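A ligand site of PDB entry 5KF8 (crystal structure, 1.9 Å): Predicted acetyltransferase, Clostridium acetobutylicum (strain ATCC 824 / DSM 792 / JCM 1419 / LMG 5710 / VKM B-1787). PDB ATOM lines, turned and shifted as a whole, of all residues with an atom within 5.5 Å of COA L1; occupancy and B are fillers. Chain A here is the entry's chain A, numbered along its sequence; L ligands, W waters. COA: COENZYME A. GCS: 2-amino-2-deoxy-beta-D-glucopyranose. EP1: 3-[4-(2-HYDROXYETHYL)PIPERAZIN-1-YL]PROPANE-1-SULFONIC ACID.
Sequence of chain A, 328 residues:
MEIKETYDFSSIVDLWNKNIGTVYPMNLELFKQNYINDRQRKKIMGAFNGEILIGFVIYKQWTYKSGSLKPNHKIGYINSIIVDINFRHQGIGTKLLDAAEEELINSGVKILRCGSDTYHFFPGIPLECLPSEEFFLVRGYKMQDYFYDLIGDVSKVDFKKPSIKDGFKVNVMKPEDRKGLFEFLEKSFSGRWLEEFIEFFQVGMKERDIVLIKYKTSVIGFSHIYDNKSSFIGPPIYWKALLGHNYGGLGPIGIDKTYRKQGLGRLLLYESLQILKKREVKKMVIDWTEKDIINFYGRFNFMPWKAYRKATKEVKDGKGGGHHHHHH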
ATOM      1  N   PHE A 189      -2.274  18.095 -36.415  1.00  0.00           N
ATOM      2  CA  PHE A 189      -2.856  17.363 -35.322  1.00  0.00           C
ATOM      3  C   PHE A 189      -4.344  17.663 -35.243  1.00  0.00           C
ATOM      4  O   PHE A 189      -4.793  18.312 -34.309  1.00  0.00           O
ATOM      5  CB  PHE A 189      -2.156  17.685 -33.991  1.00  0.00           C
ATOM      6  CG  PHE A 189      -0.692  17.350 -33.958  1.00  0.00           C
ATOM      7  CD1 PHE A 189      -0.257  16.023 -33.916  1.00  0.00           C
ATOM      8  CD2 PHE A 189       0.252  18.363 -33.994  1.00  0.00           C
ATOM      9  CE1 PHE A 189       1.082  15.709 -33.881  1.00  0.00           C
ATOM     10  CE2 PHE A 189       1.600  18.048 -34.001  1.00  0.00           C
ATOM     11  CZ  PHE A 189       2.017  16.726 -33.920  1.00  0.00           C
ATOM     12  N   TRP A 193      -6.438  16.446 -30.368  1.00  0.00           N
ATOM     13  CA  TRP A 193      -5.664  17.529 -29.794  1.00  0.00           C
ATOM     14  C   TRP A 193      -6.213  18.877 -30.258  1.00  0.00           C
ATOM     15  O   TRP A 193      -6.266  19.839 -29.472  1.00  0.00           O
ATOM     16  CB  TRP A 193      -4.180  17.349 -30.162  1.00  0.00           C
ATOM     17  CG  TRP A 193      -3.461  16.263 -29.374  1.00  0.00           C
ATOM     18  CD1 TRP A 193      -3.994  15.472 -28.407  1.00  0.00           C
ATOM     19  CD2 TRP A 193      -2.086  15.874 -29.476  1.00  0.00           C
ATOM     20  NE1 TRP A 193      -3.063  14.601 -27.916  1.00  0.00           N
ATOM     21  CE2 TRP A 193      -1.873  14.835 -28.531  1.00  0.00           C
ATOM     22  CE3 TRP A 193      -0.996  16.299 -30.270  1.00  0.00           C
ATOM     23  CZ2 TRP A 193      -0.622  14.204 -28.363  1.00  0.00           C
ATOM     24  CZ3 TRP A 193       0.246  15.671 -30.107  1.00  0.00           C
ATOM     25  CH2 TRP A 193       0.418  14.627 -29.156  1.00  0.00           C
ATOM     26  N   ILE A 253       2.373  17.343 -26.518  1.00  0.00           N
ATOM     27  CA  ILE A 253       3.520  17.997 -27.174  1.00  0.00           C
ATOM     28  C   ILE A 253       3.631  17.373 -28.585  1.00  0.00           C
ATOM     29  O   ILE A 253       3.461  16.158 -28.752  1.00  0.00           O
ATOM     30  CB  ILE A 253       4.810  17.822 -26.350  1.00  0.00           C
ATOM     31  CG1 ILE A 253       5.986  18.561 -26.965  1.00  0.00           C
ATOM     32  CG2 ILE A 253       5.172  16.367 -26.231  1.00  0.00           C
ATOM     33  CD1 ILE A 253       7.196  18.606 -26.072  1.00  0.00           C
ATOM     34  N   GLY A 254       3.825  18.208 -29.609  1.00  0.00           N
ATOM     35  CA  GLY A 254       3.987  17.721 -30.975  1.00  0.00           C
ATOM     36  C   GLY A 254       4.711  18.704 -31.864  1.00  0.00           C
ATOM     37  O   GLY A 254       4.641  19.914 -31.609  1.00  0.00           O
ATOM     38  N   ILE A 255       5.336  18.166 -32.927  1.00  0.00           N
ATOM     39  CA  ILE A 255       6.065  18.873 -33.975  1.00  0.00           C
ATOM     40  C   ILE A 255       5.541  18.394 -35.339  1.00  0.00           C
ATOM     41  O   ILE A 255       5.257  17.236 -35.542  1.00  0.00           O
ATOM     42  CB  ILE A 255       7.551  18.479 -33.894  1.00  0.00           C
ATOM     43  CG1 ILE A 255       8.152  19.020 -32.580  1.00  0.00           C
ATOM     44  CG2 ILE A 255       8.351  18.890 -35.106  1.00  0.00           C
ATOM     45  CD1 ILE A 255       8.411  20.505 -32.539  1.00  0.00           C
ATOM     46  N   TYR A 259       9.331  18.390 -39.826  1.00  0.00           N
ATOM     47  CA  TYR A 259      10.446  18.886 -38.993  1.00  0.00           C
ATOM     48  C   TYR A 259      10.982  17.905 -37.941  1.00  0.00           C
ATOM     49  O   TYR A 259      11.785  18.253 -37.075  1.00  0.00           O
ATOM     50  CB  TYR A 259      10.014  20.153 -38.238  1.00  0.00           C
ATOM     51  CG  TYR A 259       9.899  21.348 -39.142  1.00  0.00           C
ATOM     52  CD1 TYR A 259      10.954  22.223 -39.305  1.00  0.00           C
ATOM     53  CD2 TYR A 259       8.745  21.582 -39.850  1.00  0.00           C
ATOM     54  CE1 TYR A 259      10.860  23.343 -40.128  1.00  0.00           C
ATOM     55  CE2 TYR A 259       8.637  22.692 -40.678  1.00  0.00           C
ATOM     56  CZ  TYR A 259       9.697  23.571 -40.800  1.00  0.00           C
ATOM     57  OH  TYR A 259       9.584  24.653 -41.642  1.00  0.00           O
ATOM     58  N   ARG A 260      10.477  16.683 -37.978  1.00  0.00           N
ATOM     59  CA  ARG A 260      10.821  15.700 -36.957  1.00  0.00           C
ATOM     60  C   ARG A 260      12.232  15.154 -37.125  1.00  0.00           C
ATOM     61  O   ARG A 260      12.844  15.266 -38.183  1.00  0.00           O
ATOM     62  CB  ARG A 260       9.787  14.581 -36.957  1.00  0.00           C
ATOM     63  CG  ARG A 260       8.596  14.994 -36.126  1.00  0.00           C
ATOM     64  CD  ARG A 260       7.483  13.976 -36.119  1.00  0.00           C
ATOM     65  NE  ARG A 260       6.160  14.608 -35.953  1.00  0.00           N
ATOM     66  CZ  ARG A 260       5.006  13.996 -36.149  1.00  0.00           C
ATOM     67  NH1 ARG A 260       5.015  12.701 -36.475  1.00  0.00           N
ATOM     68  NH2 ARG A 260       3.831  14.637 -36.003  1.00  0.00           N
ATOM     69  N   LYS A 261      12.732  14.526 -36.071  1.00  0.00           N
ATOM     70  CA  LYS A 261      14.060  13.943 -36.085  1.00  0.00           C
ATOM     71  C   LYS A 261      15.190  14.945 -36.425  1.00  0.00           C
ATOM     72  O   LYS A 261      16.199  14.569 -37.008  1.00  0.00           O
ATOM     73  CB  LYS A 261      14.036  12.674 -36.968  1.00  0.00           C
ATOM     74  CG  LYS A 261      13.205  11.539 -36.359  1.00  0.00           C
ATOM     75  CD  LYS A 261      13.642  11.296 -34.913  1.00  0.00           C
ATOM     76  CE  LYS A 261      13.921   9.851 -34.527  1.00  0.00           C
ATOM     77  NZ  LYS A 261      12.670   9.073 -34.606  1.00  0.00           N
ATOM     78  N   GLN A 262      15.047  16.188 -35.974  1.00  0.00           N
ATOM     79  CA  GLN A 262      16.094  17.199 -36.048  1.00  0.00           C
ATOM     80  C   GLN A 262      16.479  17.760 -34.718  1.00  0.00           C
ATOM     81  O   GLN A 262      17.244  18.721 -34.687  1.00  0.00           O
ATOM     82  CB  GLN A 262      15.646  18.410 -36.832  1.00  0.00           C
ATOM     83  CG  GLN A 262      15.235  18.110 -38.237  1.00  0.00           C
ATOM     84  CD  GLN A 262      14.806  19.357 -39.001  1.00  0.00           C
ATOM     85  OE1 GLN A 262      15.140  20.500 -38.650  1.00  0.00           O
ATOM     86  NE2 GLN A 262      14.055  19.138 -40.048  1.00  0.00           N
ATOM     87  N   GLY A 263      15.947  17.236 -33.612  1.00  0.00           N
ATOM     88  CA  GLY A 263      16.269  17.803 -32.319  1.00  0.00           C
ATOM     89  C   GLY A 263      15.323  18.923 -31.918  1.00  0.00           C
ATOM     90  O   GLY A 263      15.483  19.496 -30.871  1.00  0.00           O
ATOM     91  N   LEU A 264      14.312  19.212 -32.739  1.00  0.00           N
ATOM     92  CA  LEU A 264      13.385  20.269 -32.431  1.00  0.00           C
ATOM     93  C   LEU A 264      12.376  19.899 -31.342  1.00  0.00           C
ATOM     94  O   LEU A 264      11.988  20.739 -30.552  1.00  0.00           O
ATOM     95  CB  LEU A 264      12.680  20.750 -33.685  1.00  0.00           C
ATOM     96  CG  LEU A 264      13.686  21.369 -34.690  1.00  0.00           C
ATOM     97  CD1 LEU A 264      13.025  21.614 -36.027  1.00  0.00           C
ATOM     98  CD2 LEU A 264      14.303  22.633 -34.124  1.00  0.00           C
ATOM     99  N   GLY A 265      11.938  18.650 -31.275  1.00  0.00           N
ATOM    100  CA  GLY A 265      11.119  18.197 -30.136  1.00  0.00           C
ATOM    101  C   GLY A 265      11.872  18.284 -28.830  1.00  0.00           C
ATOM    102  O   GLY A 265      11.370  18.774 -27.814  1.00  0.00           O
ATOM    103  N   ARG A 266      13.135  17.883 -28.864  1.00  0.00           N
ATOM    104  CA  ARG A 266      13.946  17.955 -27.686  1.00  0.00           C
ATOM    105  C   ARG A 266      14.112  19.431 -27.257  1.00  0.00           C
ATOM    106  O   ARG A 266      14.066  19.751 -26.076  1.00  0.00           O
ATOM    107  CB  ARG A 266      15.272  17.212 -27.955  1.00  0.00           C
ATOM    108  CG  ARG A 266      16.191  17.238 -26.769  1.00  0.00           C
ATOM    109  CD  ARG A 266      17.555  16.693 -27.130  1.00  0.00           C
ATOM    110  NE  ARG A 266      17.441  15.295 -27.570  1.00  0.00           N
ATOM    111  CZ  ARG A 266      18.472  14.552 -27.948  1.00  0.00           C
ATOM    112  NH1 ARG A 266      19.702  15.050 -27.907  1.00  0.00           N
ATOM    113  NH2 ARG A 266      18.259  13.292 -28.332  1.00  0.00           N
ATOM    114  N   LEU A 267      14.313  20.343 -28.202  1.00  0.00           N
ATOM    115  CA  LEU A 267      14.417  21.760 -27.870  1.00  0.00           C
ATOM    116  C   LEU A 267      13.106  22.280 -27.232  1.00  0.00           C
ATOM    117  O   LEU A 267      13.152  23.014 -26.272  1.00  0.00           O
ATOM    118  CB  LEU A 267      14.754  22.587 -29.087  1.00  0.00           C
ATOM    119  CG  LEU A 267      14.837  24.100 -28.817  1.00  0.00           C
ATOM    120  CD1 LEU A 267      15.988  24.444 -27.878  1.00  0.00           C
ATOM    121  CD2 LEU A 267      14.814  24.841 -30.185  1.00  0.00           C
ATOM    122  N   ASP A 287       1.552  12.822 -18.912  1.00  0.00           N
ATOM    123  CA  ASP A 287       0.483  11.834 -18.819  1.00  0.00           C
ATOM    124  C   ASP A 287       0.382  11.022 -20.122  1.00  0.00           C
ATOM    125  O   ASP A 287       0.697  11.527 -21.199  1.00  0.00           O
ATOM    126  CB  ASP A 287      -0.879  12.515 -18.559  1.00  0.00           C
ATOM    127  CG  ASP A 287      -1.380  13.321 -19.762  1.00  0.00           C
ATOM    128  OD1 ASP A 287      -0.696  14.295 -20.128  1.00  0.00           O
ATOM    129  OD2 ASP A 287      -2.363  12.906 -20.428  1.00  0.00           O
ATOM    130  N   TRP A 288      -0.142   9.800 -20.027  1.00  0.00           N
ATOM    131  CA  TRP A 288      -0.558   8.997 -21.201  1.00  0.00           C
ATOM    132  C   TRP A 288       0.464   9.013 -22.365  1.00  0.00           C
ATOM    133  O   TRP A 288       0.208   9.536 -23.491  1.00  0.00           O
ATOM    134  CB  TRP A 288      -1.919   9.507 -21.638  1.00  0.00           C
ATOM    135  CG  TRP A 288      -2.736   8.601 -22.566  1.00  0.00           C
ATOM    136  CD1 TRP A 288      -2.288   7.520 -23.213  1.00  0.00           C
ATOM    137  CD2 TRP A 288      -4.114   8.763 -22.968  1.00  0.00           C
ATOM    138  NE1 TRP A 288      -3.260   6.976 -23.991  1.00  0.00           N
ATOM    139  CE2 TRP A 288      -4.395   7.741 -23.888  1.00  0.00           C
ATOM    140  CE3 TRP A 288      -5.135   9.682 -22.646  1.00  0.00           C
ATOM    141  CZ2 TRP A 288      -5.659   7.552 -24.468  1.00  0.00           C
ATOM    142  CZ3 TRP A 288      -6.371   9.536 -23.241  1.00  0.00           C
ATOM    143  CH2 TRP A 288      -6.637   8.477 -24.151  1.00  0.00           C
ATOM    144  N   THR A 289       1.593   8.394 -22.066  1.00  0.00           N
ATOM    145  CA  THR A 289       2.683   8.099 -22.997  1.00  0.00           C
ATOM    146  C   THR A 289       2.753   6.642 -23.471  1.00  0.00           C
ATOM    147  O   THR A 289       2.365   5.732 -22.798  1.00  0.00           O
ATOM    148  CB  THR A 289       4.059   8.495 -22.432  1.00  0.00           C
ATOM    149  OG1 THR A 289       4.481   7.657 -21.316  1.00  0.00           O
ATOM    150  CG2 THR A 289       3.989   9.905 -21.952  1.00  0.00           C
ATOM    151  N   GLU A 290       3.322   6.434 -24.656  1.00  0.00           N
ATOM    152  CA  GLU A 290       3.550   5.073 -25.140  1.00  0.00           C
ATOM    153  C   GLU A 290       4.936   4.637 -24.709  1.00  0.00           C
ATOM    154  O   GLU A 290       5.841   5.459 -24.480  1.00  0.00           O
ATOM    155  CB  GLU A 290       3.503   5.043 -26.665  1.00  0.00           C
ATOM    156  CG  GLU A 290       2.301   5.719 -27.246  1.00  0.00           C
ATOM    157  CD  GLU A 290       1.690   4.924 -28.361  1.00  0.00           C
ATOM    158  OE1 GLU A 290       1.913   5.288 -29.524  1.00  0.00           O
ATOM    159  OE2 GLU A 290       0.985   3.947 -28.050  1.00  0.00           O
ATOM    160  N   ILE A 293       8.141   6.111 -26.529  1.00  0.00           N
ATOM    161  CA  ILE A 293       8.507   7.521 -26.360  1.00  0.00           C
ATOM    162  C   ILE A 293       9.067   7.821 -24.964  1.00  0.00           C
ATOM    163  O   ILE A 293       9.446   8.963 -24.654  1.00  0.00           O
ATOM    164  CB  ILE A 293       7.317   8.482 -26.690  1.00  0.00           C
ATOM    165  CG1 ILE A 293       7.761   9.914 -27.012  1.00  0.00           C
ATOM    166  CG2 ILE A 293       6.369   8.579 -25.498  1.00  0.00           C
ATOM    167  CD1 ILE A 293       8.738   9.995 -28.173  1.00  0.00           C
ATOM    168  N   PHE A 296      12.502   9.619 -24.572  1.00  0.00           N
ATOM    169  CA  PHE A 296      12.506  11.032 -24.974  1.00  0.00           C
ATOM    170  C   PHE A 296      12.346  11.933 -23.745  1.00  0.00           C
ATOM    171  O   PHE A 296      13.080  12.926 -23.529  1.00  0.00           O
ATOM    172  CB  PHE A 296      11.373  11.220 -25.955  1.00  0.00           C
ATOM    173  CG  PHE A 296      11.102  12.654 -26.342  1.00  0.00           C
ATOM    174  CD1 PHE A 296      12.009  13.352 -27.082  1.00  0.00           C
ATOM    175  CD2 PHE A 296       9.884  13.277 -25.987  1.00  0.00           C
ATOM    176  CE1 PHE A 296      11.713  14.665 -27.457  1.00  0.00           C
ATOM    177  CE2 PHE A 296       9.581  14.579 -26.380  1.00  0.00           C
ATOM    178  CZ  PHE A 296      10.539  15.292 -27.090  1.00  0.00           C
ATOM    179  N   TYR A 297      11.429  11.538 -22.860  1.00  0.00           N
ATOM    180  CA  TYR A 297      11.248  12.287 -21.630  1.00  0.00           C
ATOM    181  C   TYR A 297      12.292  11.870 -20.582  1.00  0.00           C
ATOM    182  O   TYR A 297      12.687  12.666 -19.753  1.00  0.00           O
ATOM    183  CB  TYR A 297       9.826  12.032 -21.101  1.00  0.00           C
ATOM    184  CG  TYR A 297       8.702  12.452 -22.037  1.00  0.00           C
ATOM    185  CD1 TYR A 297       8.406  13.792 -22.221  1.00  0.00           C
ATOM    186  CD2 TYR A 297       7.940  11.525 -22.734  1.00  0.00           C
ATOM    187  CE1 TYR A 297       7.389  14.193 -23.075  1.00  0.00           C
ATOM    188  CE2 TYR A 297       6.917  11.927 -23.575  1.00  0.00           C
ATOM    189  CZ  TYR A 297       6.640  13.250 -23.741  1.00  0.00           C
ATOM    190  OH  TYR A 297       5.591  13.661 -24.548  1.00  0.00           O
HETATM  191  O5B COA L   1      13.429  16.419 -31.423  1.00  0.00           O
HETATM  192  P1A COA L   1      13.717  14.937 -31.467  1.00  0.00           P
HETATM  193  O1A COA L   1      14.403  14.262 -30.299  1.00  0.00           O
HETATM  194  O2A COA L   1      14.556  14.626 -32.798  1.00  0.00           O
HETATM  195  O3A COA L   1      12.324  14.168 -31.735  1.00  0.00           O
HETATM  196  P2A COA L   1      11.222  14.789 -32.726  1.00  0.00           P
HETATM  197  O4A COA L   1      11.803  16.038 -33.361  1.00  0.00           O
HETATM  198  O5A COA L   1      10.686  13.687 -33.596  1.00  0.00           O
HETATM  199  O6A COA L   1      10.054  15.242 -31.717  1.00  0.00           O
HETATM  200  CBP COA L   1       7.959  14.410 -30.850  1.00  0.00           C
HETATM  201  CCP COA L   1       9.485  14.301 -30.810  1.00  0.00           C
HETATM  202  CDP COA L   1       7.342  13.322 -29.978  1.00  0.00           C
HETATM  203  CEP COA L   1       7.529  15.786 -30.357  1.00  0.00           C
HETATM  204  CAP COA L   1       7.493  14.220 -32.287  1.00  0.00           C
HETATM  205  OAP COA L   1       7.917  12.946 -32.772  1.00  0.00           O
HETATM  206  C9P COA L   1       5.998  14.308 -32.334  1.00  0.00           C
HETATM  207  O9P COA L   1       5.434  15.386 -32.317  1.00  0.00           O
HETATM  208  N8P COA L   1       5.343  13.150 -32.399  1.00  0.00           N
HETATM  209  C7P COA L   1       3.922  13.097 -32.645  1.00  0.00           C
HETATM  210  C6P COA L   1       3.103  13.522 -31.420  1.00  0.00           C
HETATM  211  C5P COA L   1       3.461  12.631 -30.249  1.00  0.00           C
HETATM  212  O5P COA L   1       3.331  11.416 -30.328  1.00  0.00           O
HETATM  213  N4P COA L   1       3.922  13.245 -29.164  1.00  0.00           N
HETATM  214  C3P COA L   1       4.205  12.512 -27.944  1.00  0.00           C
HETATM  215  C2P COA L   1       2.992  12.393 -27.041  1.00  0.00           C
HETATM  216  S1P COA L   1       3.459  11.571 -25.501  1.00  0.00           S
HETATM  217  C1  GCS L   2      -1.283  11.850 -25.267  1.00  0.00           C
HETATM  218  C2  GCS L   2      -0.509  12.907 -24.502  1.00  0.00           C
HETATM  219  C3  GCS L   2      -1.327  13.458 -23.356  1.00  0.00           C
HETATM  220  C4  GCS L   2      -2.808  13.758 -23.672  1.00  0.00           C
HETATM  221  C5  GCS L   2      -3.401  12.563 -24.416  1.00  0.00           C
HETATM  222  C6  GCS L   2      -4.835  12.680 -24.962  1.00  0.00           C
HETATM  223  N2  GCS L   2       0.724  12.339 -24.006  1.00  0.00           N
HETATM  224  O1  GCS L   2      -0.606  11.405 -26.444  1.00  0.00           O
HETATM  225  O3  GCS L   2      -0.647  14.607 -22.825  1.00  0.00           O
HETATM  226  O4  GCS L   2      -3.594  14.042 -22.517  1.00  0.00           O
HETATM  227  O5  GCS L   2      -2.601  12.320 -25.586  1.00  0.00           O
HETATM  228  O6  GCS L   2      -4.968  13.785 -25.887  1.00  0.00           O
HETATM  229  O2S EP1 L   3      -4.961  15.269 -32.529  1.00  0.00           O
HETATM  230  S   EP1 L   3      -4.571  14.050 -33.161  1.00  0.00           S
HETATM  231  O3S EP1 L   3      -5.631  13.137 -32.855  1.00  0.00           O
HETATM  232  O1S EP1 L   3      -4.413  14.170 -34.768  1.00  0.00           O
HETATM  233  C11 EP1 L   3      -3.066  13.509 -32.701  1.00  0.00           C
HETATM  234  C10 EP1 L   3      -3.275  12.434 -31.670  1.00  0.00           C
HETATM  235  C9  EP1 L   3      -1.901  12.016 -31.199  1.00  0.00           C
HETATM  236  N1  EP1 L   3      -1.991  11.163 -29.993  1.00  0.00           N
HETATM  237  C2  EP1 L   3      -3.340  10.787 -29.478  1.00  0.00           C
HETATM  238  C3  EP1 L   3      -3.267  10.102 -28.110  1.00  0.00           C
HETATM  239  N4  EP1 L   3      -2.221   9.023 -28.127  1.00  0.00           N
HETATM  240  C5  EP1 L   3      -0.980   9.262 -28.907  1.00  0.00           C
HETATM  241  C6  EP1 L   3      -1.112  10.028 -30.204  1.00  0.00           C
HETATM  242  C7  EP1 L   3      -1.982   8.463 -26.785  1.00  0.00           C
HETATM  243  C8  EP1 L   3      -0.694   7.663 -26.626  1.00  0.00           C
HETATM  244  O8  EP1 L   3       0.298   8.494 -26.039  1.00  0.00           O
HETATM  245  O   HOH W   1       2.799  14.321 -23.511  1.00  0.00           O
HETATM  246  O   HOH W   2       1.814  10.436 -32.250  1.00  0.00           O
HETATM  247  O   HOH W   3       2.919   8.811 -26.470  1.00  0.00           O
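A nitrogen (N2) of GCS L2 lies close to a sulfur (S1P) of COA L1.
An oxygen (O1) of GCS L2 lies within hydrogen-bond range of an oxygen (O8) of EP1 L3.
The side-chain carboxylate (OD2) of Asp 287 lies within hydrogen-bond range of an oxygen (O4) of GCS L2 (2.7 Å).
N of Gly 263 lies within hydrogen-bond range of O2A of COA L1, at 3.1 Å.
N of Ile 255 is in hydrogen-bond range of O9P of COA L1 (2.8 Å).
N4P of COA L1 sits at hydrogen-bond distance from O of Ile 253.
An oxygen (O6) of GCS L2 is in hydrogen-bond range of the indole nitrogen (NE1) of Trp 193 (2.9 Å).
The backbone carbonyl oxygen (O) of Trp 288 is in hydrogen-bond range of an oxygen (O8) of EP1 L3 (2.8 Å).
An oxygen (O5B) of COA L1 lies within hydrogen-bond range of the backbone NH (N) of Arg 266 (3.0 Å).
The backbone NH of Lys 261 lies within hydrogen-bond range of an oxygen (O4A) of COA L1, at 3.2 Å.
A nitrogen (N2) of GCS L2 sits at hydrogen-bond distance from the backbone carbonyl oxygen (O) of Asp 287, at 2.9 Å.
OH of Tyr 297 lies close to S1P of COA L1.
The backbone NH of Gly 265 is in hydrogen-bond range of an oxygen (O5B) of COA L1.
The backbone NH of Trp 193 lies within hydrogen-bond range of an oxygen (O2S) of EP1 L3 (2.9 Å).
The backbone carbonyl oxygen of Trp 288 lies within hydrogen-bond range of a nitrogen (N2) of GCS L2.
N of Leu 264 is in hydrogen-bond range of O5B of COA L1 (3.2 Å).
The backbone carbonyl oxygen (O) of Ile 255 is in hydrogen-bond range of the guanidinium group (NE) of Arg 260 (2.8 Å).
Water W3 lies within hydrogen-bond range of an oxygen (O8) of EP1 L3 (2.7 Å), a sulfur (S1P) of COA L1 (3.0 Å) and the backbone NH of Glu 290 (3.0 Å).
Water W1 lies within hydrogen-bond range of a nitrogen (N2) of GCS L2 (2.9 Å), the side-chain hydroxyl of Tyr 297 (3.1 Å) and a sulfur (S1P) of COA L1 (3.5 Å).
Merely in contact with COA L1: Gly 254, Arg 260, Gln 262, Trp 193, Phe 189, Phe 296 and Thr 289.
Hydrophobic or aromatic side chains that line COA L1: Phe 189, Trp 193, Ile 255, Phe 296 and Tyr 297.
15 residues have an atom within 4 Å of COA L1: Phe 189, Trp 193, Ile 253, Gly 254, Ile 255, Arg 260, Lys 261, Gln 262, Gly 263, Leu 264, Gly 265, Arg 266, Thr 289, Phe 296 and Tyr 297.
The nearest printed residue that does not touch COA L1 is Ile 293 (4.03 Å).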
